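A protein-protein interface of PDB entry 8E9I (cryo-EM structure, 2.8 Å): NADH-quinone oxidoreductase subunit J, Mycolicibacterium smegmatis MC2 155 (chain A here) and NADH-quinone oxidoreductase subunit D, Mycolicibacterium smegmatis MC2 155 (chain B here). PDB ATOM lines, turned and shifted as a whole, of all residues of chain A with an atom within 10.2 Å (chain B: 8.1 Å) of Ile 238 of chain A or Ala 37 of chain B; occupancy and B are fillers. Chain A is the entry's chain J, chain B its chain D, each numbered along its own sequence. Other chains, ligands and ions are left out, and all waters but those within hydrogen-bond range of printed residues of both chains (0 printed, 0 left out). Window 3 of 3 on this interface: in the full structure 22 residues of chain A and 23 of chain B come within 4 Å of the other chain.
NH1 of Arg 40 of chain B lies within hydrogen-bond range of OG1 of Thr 68 of chain B (2.6 Å).
Among the printed residues, pairs that only touch across the chains: Leu 207 of chain A with Arg 71 of chain B (3.4 Å), Val 219 of chain A with Val 42 of chain B (3.7 Å), Val 235 of chain A with Arg 71 of chain B (3.8 Å), Ser 236 of chain A with Arg 71 of chain B (3.5 Å), Ile 238 of chain A with Ala 37 of chain B (3.6 Å), Ile 238 of chain A with Arg 40 of chain B (3.6 Å) and Leu 239 of chain A with Val 42 of chain B (3.96 Å).
Ile 238 of chain A touches just these residues of chain B: Ala 37 and Arg 40.
Ala 37 of chain B touches just one residue of chain A: Ile 238 (3.6 Å).
No residue of chain B comes within 4 Å of Thr 237 of chain A.
No residue of chain A comes within 4 Å of Gln 36 of chain B.
Printed residues of chain B within 4 Å of Ser 236 of chain A: Arg 71 (3.5 Å).
Of the printed residues of chain B, Ser 234 of chain A touches Arg 71.
Of the printed residues of chain A, Val 42 of chain B touches Val 219 and Leu 239.
Pro 232 of chain A touches none of the printed residues of chain B.
The nearest residue of chain A that does not touch Ala 37 of chain B is Leu 239 of chain A (5.8 Å).
The nearest printed residue of chain B that does not touch Leu 233 of chain A is Glu 61 of chain B (10.2 Å).
Hydrophobic or aromatic side chains of chain A that line the printed part of chain B: Leu 207, Val 219, Ile 238 and Leu 239.
Of the 13 printed residues of chain B, 4 touch a printed residue of chain A.
Printed residues of chain B that touch a printed residue of chain A: Ala 37, Arg 40, Val 42 and Arg 71.
Hydrophobic or aromatic side chains of chain B within 4 Å of the printed part of chain A: Ala 37 and Val 42.
Among the printed residues, 9 pairs touch across the chains.
Among the printed residues, no Asp or Glu carboxylate lies within 4 Å of a Lys or Arg side-chain nitrogen of the other chain.
The backbone carbonyl oxygen of Leu 233 of chain A sits at hydrogen-bond distance from the guanidinium group of Arg 71 of chain B.
The backbone carbonyl oxygen (O) of Ser 234 of chain A lies within hydrogen-bond range of the guanidinium group (NE) of Arg 71 of chain B, at 3.1 Å.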
ATOM      1  N   LEU A 207     -15.732   3.521  34.546  1.00  0.00           N
ATOM      2  CA  LEU A 207     -16.727   2.436  34.700  1.00  0.00           C
ATOM      3  C   LEU A 207     -16.046   1.077  34.552  1.00  0.00           C
ATOM      4  O   LEU A 207     -15.122   0.952  33.745  1.00  0.00           O
ATOM      5  CB  LEU A 207     -17.845   2.638  33.678  1.00  0.00           C
ATOM      6  CG  LEU A 207     -19.005   3.506  34.152  1.00  0.00           C
ATOM      7  CD1 LEU A 207     -19.985   3.752  33.019  1.00  0.00           C
ATOM      8  CD2 LEU A 207     -19.710   2.853  35.327  1.00  0.00           C
ATOM      9  N   VAL A 219     -16.996  -7.361  24.426  1.00  0.00           N
ATOM     10  CA  VAL A 219     -17.487  -6.241  25.220  1.00  0.00           C
ATOM     11  C   VAL A 219     -18.885  -6.467  25.765  1.00  0.00           C
ATOM     12  O   VAL A 219     -19.245  -5.870  26.784  1.00  0.00           O
ATOM     13  CB  VAL A 219     -17.471  -4.949  24.382  1.00  0.00           C
ATOM     14  CG1 VAL A 219     -16.062  -4.625  23.936  1.00  0.00           C
ATOM     15  CG2 VAL A 219     -18.383  -5.086  23.183  1.00  0.00           C
ATOM     16  N   ASP A 220     -19.685  -7.309  25.118  1.00  0.00           N
ATOM     17  CA  ASP A 220     -21.054  -7.548  25.554  1.00  0.00           C
ATOM     18  C   ASP A 220     -21.143  -8.401  26.810  1.00  0.00           C
ATOM     19  O   ASP A 220     -22.242  -8.559  27.349  1.00  0.00           O
ATOM     20  CB  ASP A 220     -21.841  -8.224  24.431  1.00  0.00           C
ATOM     21  N   PRO A 232     -24.426  -4.855  36.355  1.00  0.00           N
ATOM     22  CA  PRO A 232     -24.980  -4.058  35.251  1.00  0.00           C
ATOM     23  C   PRO A 232     -24.023  -3.009  34.724  1.00  0.00           C
ATOM     24  O   PRO A 232     -24.032  -2.733  33.519  1.00  0.00           O
ATOM     25  CB  PRO A 232     -26.223  -3.412  35.877  1.00  0.00           C
ATOM     26  CG  PRO A 232     -26.568  -4.291  37.029  1.00  0.00           C
ATOM     27  CD  PRO A 232     -25.264  -4.769  37.561  1.00  0.00           C
ATOM     28  N   LEU A 233     -23.196  -2.420  35.585  1.00  0.00           N
ATOM     29  CA  LEU A 233     -22.317  -1.341  35.161  1.00  0.00           C
ATOM     30  C   LEU A 233     -21.205  -1.816  34.238  1.00  0.00           C
ATOM     31  O   LEU A 233     -20.756  -1.045  33.385  1.00  0.00           O
ATOM     32  CB  LEU A 233     -21.717  -0.663  36.389  1.00  0.00           C
ATOM     33  CG  LEU A 233     -22.748  -0.087  37.358  1.00  0.00           C
ATOM     34  CD1 LEU A 233     -22.059   0.516  38.565  1.00  0.00           C
ATOM     35  CD2 LEU A 233     -23.613   0.946  36.660  1.00  0.00           C
ATOM     36  N   SER A 234     -20.749  -3.060  34.386  1.00  0.00           N
ATOM     37  CA  SER A 234     -19.639  -3.545  33.577  1.00  0.00           C
ATOM     38  C   SER A 234     -19.985  -3.524  32.097  1.00  0.00           C
ATOM     39  O   SER A 234     -19.157  -3.144  31.263  1.00  0.00           O
ATOM     40  CB  SER A 234     -19.255  -4.957  34.012  1.00  0.00           C
ATOM     41  OG  SER A 234     -20.354  -5.838  33.880  1.00  0.00           O
ATOM     42  N   VAL A 235     -21.201  -3.940  31.752  1.00  0.00           N
ATOM     43  CA  VAL A 235     -21.639  -3.894  30.364  1.00  0.00           C
ATOM     44  C   VAL A 235     -22.262  -2.538  30.076  1.00  0.00           C
ATOM     45  O   VAL A 235     -23.056  -2.016  30.869  1.00  0.00           O
ATOM     46  CB  VAL A 235     -22.623  -5.037  30.068  1.00  0.00           C
ATOM     47  CG1 VAL A 235     -23.819  -4.982  31.010  1.00  0.00           C
ATOM     48  CG2 VAL A 235     -23.077  -4.973  28.621  1.00  0.00           C
ATOM     49  N   SER A 236     -21.901  -1.959  28.936  1.00  0.00           N
ATOM     50  CA  SER A 236     -22.396  -0.637  28.581  1.00  0.00           C
ATOM     51  C   SER A 236     -23.917  -0.597  28.629  1.00  0.00           C
ATOM     52  O   SER A 236     -24.588  -1.633  28.603  1.00  0.00           O
ATOM     53  CB  SER A 236     -21.910  -0.249  27.186  1.00  0.00           C
ATOM     54  OG  SER A 236     -22.378   1.039  26.834  1.00  0.00           O
ATOM     55  N   THR A 237     -24.463   0.615  28.718  1.00  0.00           N
ATOM     56  CA  THR A 237     -25.911   0.767  28.760  1.00  0.00           C
ATOM     57  C   THR A 237     -26.560   0.312  27.459  1.00  0.00           C
ATOM     58  O   THR A 237     -27.652  -0.266  27.478  1.00  0.00           O
ATOM     59  CB  THR A 237     -26.276   2.222  29.048  1.00  0.00           C
ATOM     60  N   ILE A 238     -25.904   0.554  26.322  1.00  0.00           N
ATOM     61  CA  ILE A 238     -26.523   0.307  25.023  1.00  0.00           C
ATOM     62  C   ILE A 238     -26.541  -1.159  24.628  1.00  0.00           C
ATOM     63  O   ILE A 238     -27.288  -1.531  23.716  1.00  0.00           O
ATOM     64  CB  ILE A 238     -25.795   1.100  23.923  1.00  0.00           C
ATOM     65  CG1 ILE A 238     -24.331   0.659  23.818  1.00  0.00           C
ATOM     66  CG2 ILE A 238     -25.874   2.582  24.218  1.00  0.00           C
ATOM     67  CD1 ILE A 238     -23.613   1.215  22.615  1.00  0.00           C
ATOM     68  N   LEU A 239     -25.758  -1.985  25.267  1.00  0.00           N
ATOM     69  CA  LEU A 239     -25.717  -3.360  24.796  1.00  0.00           C
ATOM     70  C   LEU A 239     -26.893  -4.163  25.343  1.00  0.00           C
ATOM     71  O   LEU A 239     -27.396  -3.878  26.434  1.00  0.00           O
ATOM     72  CB  LEU A 239     -24.406  -4.021  25.202  1.00  0.00           C
ATOM     73  CG  LEU A 239     -23.213  -3.445  24.439  1.00  0.00           C
ATOM     74  CD1 LEU A 239     -21.902  -3.736  25.152  1.00  0.00           C
ATOM     75  CD2 LEU A 239     -23.193  -4.003  23.025  1.00  0.00           C
ATOM     76  N   PRO A 240     -27.347  -5.168  24.592  1.00  0.00           N
ATOM     77  CA  PRO A 240     -28.544  -5.913  24.994  1.00  0.00           C
ATOM     78  C   PRO A 240     -28.248  -7.059  25.945  1.00  0.00           C
ATOM     79  O   PRO A 240     -28.740  -8.173  25.747  1.00  0.00           O
ATOM     80  CB  PRO A 240     -29.074  -6.430  23.654  1.00  0.00           C
ATOM     81  CG  PRO A 240     -27.816  -6.724  22.906  1.00  0.00           C
ATOM     82  CD  PRO A 240     -26.860  -5.611  23.273  1.00  0.00           C
ATOM     83  N   HIS A 241     -27.460  -6.804  26.977  1.00  0.00           N
ATOM     84  CA  HIS A 241     -27.088  -7.858  27.922  1.00  0.00           C
ATOM     85  C   HIS A 241     -26.344  -8.949  27.146  1.00  0.00           C
ATOM     86  O   HIS A 241     -25.709  -8.675  26.122  1.00  0.00           O
ATOM     87  CB  HIS A 241     -28.331  -8.329  28.653  1.00  0.00           C
ATOM     88  N   ARG A 242     -26.405 -10.192  27.614  1.00  0.00           N
ATOM     89  CA  ARG A 242     -25.710 -11.290  26.946  1.00  0.00           C
ATOM     90  C   ARG A 242     -26.252 -12.644  27.380  1.00  0.00           C
ATOM     91  O   ARG A 242     -26.145 -13.023  28.544  1.00  0.00           O
ATOM     92  CB  ARG A 242     -24.209 -11.218  27.229  1.00  0.00           C
ATOM     93  N   GLN B  36     -30.016   7.604  21.304  1.00  0.00           N
ATOM     94  CA  GLN B  36     -29.975   6.391  22.110  1.00  0.00           C
ATOM     95  C   GLN B  36     -29.019   5.375  21.493  1.00  0.00           C
ATOM     96  O   GLN B  36     -28.097   5.744  20.768  1.00  0.00           O
ATOM     97  CB  GLN B  36     -31.375   5.789  22.244  1.00  0.00           C
ATOM     98  N   ALA B  37     -29.233   4.097  21.797  1.00  0.00           N
ATOM     99  CA  ALA B  37     -28.479   3.042  21.138  1.00  0.00           C
ATOM    100  C   ALA B  37     -28.915   2.925  19.683  1.00  0.00           C
ATOM    101  O   ALA B  37     -30.084   3.125  19.341  1.00  0.00           O
ATOM    102  CB  ALA B  37     -28.675   1.708  21.853  1.00  0.00           C
ATOM    103  N   GLY B  38     -27.960   2.583  18.821  1.00  0.00           N
ATOM    104  CA  GLY B  38     -28.128   2.652  17.393  1.00  0.00           C
ATOM    105  C   GLY B  38     -27.242   3.691  16.742  1.00  0.00           C
ATOM    106  O   GLY B  38     -26.907   3.559  15.560  1.00  0.00           O
ATOM    107  N   GLU B  39     -26.842   4.713  17.498  1.00  0.00           N
ATOM    108  CA  GLU B  39     -25.924   5.735  17.023  1.00  0.00           C
ATOM    109  C   GLU B  39     -24.556   5.668  17.687  1.00  0.00           C
ATOM    110  O   GLU B  39     -23.659   6.415  17.286  1.00  0.00           O
ATOM    111  CB  GLU B  39     -26.526   7.128  17.252  1.00  0.00           C
ATOM    112  N   ARG B  40     -24.375   4.807  18.685  1.00  0.00           N
ATOM    113  CA  ARG B  40     -23.099   4.645  19.367  1.00  0.00           C
ATOM    114  C   ARG B  40     -22.552   3.253  19.087  1.00  0.00           C
ATOM    115  O   ARG B  40     -23.273   2.260  19.219  1.00  0.00           O
ATOM    116  CB  ARG B  40     -23.246   4.853  20.873  1.00  0.00           C
ATOM    117  CG  ARG B  40     -23.599   6.265  21.298  1.00  0.00           C
ATOM    118  CD  ARG B  40     -23.534   6.386  22.813  1.00  0.00           C
ATOM    119  NE  ARG B  40     -24.264   7.537  23.327  1.00  0.00           N
ATOM    120  CZ  ARG B  40     -23.827   8.788  23.278  1.00  0.00           C
ATOM    121  NH1 ARG B  40     -22.663   9.094  22.734  1.00  0.00           N
ATOM    122  NH2 ARG B  40     -24.578   9.757  23.790  1.00  0.00           N
ATOM    123  N   ILE B  41     -21.281   3.187  18.704  1.00  0.00           N
ATOM    124  CA  ILE B  41     -20.590   1.915  18.556  1.00  0.00           C
ATOM    125  C   ILE B  41     -19.791   1.626  19.821  1.00  0.00           C
ATOM    126  O   ILE B  41     -19.422   2.525  20.574  1.00  0.00           O
ATOM    127  CB  ILE B  41     -19.678   1.926  17.318  1.00  0.00           C
ATOM    128  CG1 ILE B  41     -20.444   2.434  16.099  1.00  0.00           C
ATOM    129  CG2 ILE B  41     -19.103   0.546  17.061  1.00  0.00           C
ATOM    130  CD1 ILE B  41     -20.287   3.920  15.863  1.00  0.00           C
ATOM    131  N   VAL B  42     -19.527   0.347  20.061  1.00  0.00           N
ATOM    132  CA  VAL B  42     -18.645  -0.077  21.141  1.00  0.00           C
ATOM    133  C   VAL B  42     -17.472  -0.816  20.520  1.00  0.00           C
ATOM    134  O   VAL B  42     -17.660  -1.825  19.832  1.00  0.00           O
ATOM    135  CB  VAL B  42     -19.373  -0.959  22.171  1.00  0.00           C
ATOM    136  CG1 VAL B  42     -20.050  -2.135  21.496  1.00  0.00           C
ATOM    137  CG2 VAL B  42     -18.399  -1.436  23.226  1.00  0.00           C
ATOM    138  N   VAL B  43     -16.267  -0.315  20.759  1.00  0.00           N
ATOM    139  CA  VAL B  43     -15.073  -0.800  20.085  1.00  0.00           C
ATOM    140  C   VAL B  43     -14.010  -1.096  21.129  1.00  0.00           C
ATOM    141  O   VAL B  43     -14.049  -0.564  22.241  1.00  0.00           O
ATOM    142  CB  VAL B  43     -14.558   0.225  19.052  1.00  0.00           C
ATOM    143  CG1 VAL B  43     -14.173   1.518  19.736  1.00  0.00           C
ATOM    144  CG2 VAL B  43     -13.385  -0.332  18.274  1.00  0.00           C
ATOM    145  N   LEU B  60     -14.241   1.506  24.235  1.00  0.00           N
ATOM    146  CA  LEU B  60     -14.751   2.846  23.978  1.00  0.00           C
ATOM    147  C   LEU B  60     -16.161   2.766  23.418  1.00  0.00           C
ATOM    148  O   LEU B  60     -16.400   2.075  22.422  1.00  0.00           O
ATOM    149  CB  LEU B  60     -13.843   3.600  23.011  1.00  0.00           C
ATOM    150  CG  LEU B  60     -12.360   3.640  23.365  1.00  0.00           C
ATOM    151  CD1 LEU B  60     -11.616   4.518  22.384  1.00  0.00           C
ATOM    152  CD2 LEU B  60     -12.163   4.135  24.779  1.00  0.00           C
ATOM    153  N   GLU B  61     -17.088   3.458  24.070  1.00  0.00           N
ATOM    154  CA  GLU B  61     -18.382   3.738  23.467  1.00  0.00           C
ATOM    155  C   GLU B  61     -18.302   5.079  22.758  1.00  0.00           C
ATOM    156  O   GLU B  61     -18.142   6.121  23.398  1.00  0.00           O
ATOM    157  CB  GLU B  61     -19.477   3.758  24.529  1.00  0.00           C
ATOM    158  N   ILE B  62     -18.402   5.053  21.433  1.00  0.00           N
ATOM    159  CA  ILE B  62     -18.098   6.206  20.597  1.00  0.00           C
ATOM    160  C   ILE B  62     -19.334   6.574  19.793  1.00  0.00           C
ATOM    161  O   ILE B  62     -19.942   5.714  19.148  1.00  0.00           O
ATOM    162  CB  ILE B  62     -16.901   5.922  19.671  1.00  0.00           C
ATOM    163  CG1 ILE B  62     -17.229   4.809  18.676  1.00  0.00           C
ATOM    164  CG2 ILE B  62     -15.696   5.528  20.495  1.00  0.00           C
ATOM    165  CD1 ILE B  62     -16.057   4.397  17.822  1.00  0.00           C
ATOM    166  N   THR B  68     -17.604   8.536  24.137  1.00  0.00           N
ATOM    167  CA  THR B  68     -18.682   8.779  25.086  1.00  0.00           C
ATOM    168  C   THR B  68     -18.364   8.183  26.455  1.00  0.00           C
ATOM    169  O   THR B  68     -18.569   8.834  27.481  1.00  0.00           O
ATOM    170  CB  THR B  68     -19.994   8.210  24.549  1.00  0.00           C
ATOM    171  OG1 THR B  68     -20.153   8.592  23.180  1.00  0.00           O
ATOM    172  CG2 THR B  68     -21.170   8.745  25.342  1.00  0.00           C
ATOM    173  N   ARG B  71     -14.244   2.606  29.185  1.00  0.00           N
ATOM    174  CA  ARG B  71     -13.938   1.563  30.147  1.00  0.00           C
ATOM    175  C   ARG B  71     -12.512   1.078  29.940  1.00  0.00           C
ATOM    176  O   ARG B  71     -11.987   1.085  28.827  1.00  0.00           O
ATOM    177  CB  ARG B  71     -14.919   0.406  30.005  1.00  0.00           C
ATOM    178  CG  ARG B  71     -16.288   0.714  30.554  1.00  0.00           C
ATOM    179  CD  ARG B  71     -17.243  -0.433  30.356  1.00  0.00           C
ATOM    180  NE  ARG B  71     -18.528  -0.147  30.977  1.00  0.00           N
ATOM    181  CZ  ARG B  71     -19.453   0.641  30.449  1.00  0.00           C
ATOM    182  NH1 ARG B  71     -19.285   1.208  29.266  1.00  0.00           N
ATOM    183  NH2 ARG B  71     -20.574   0.870  31.126  1.00  0.00           N
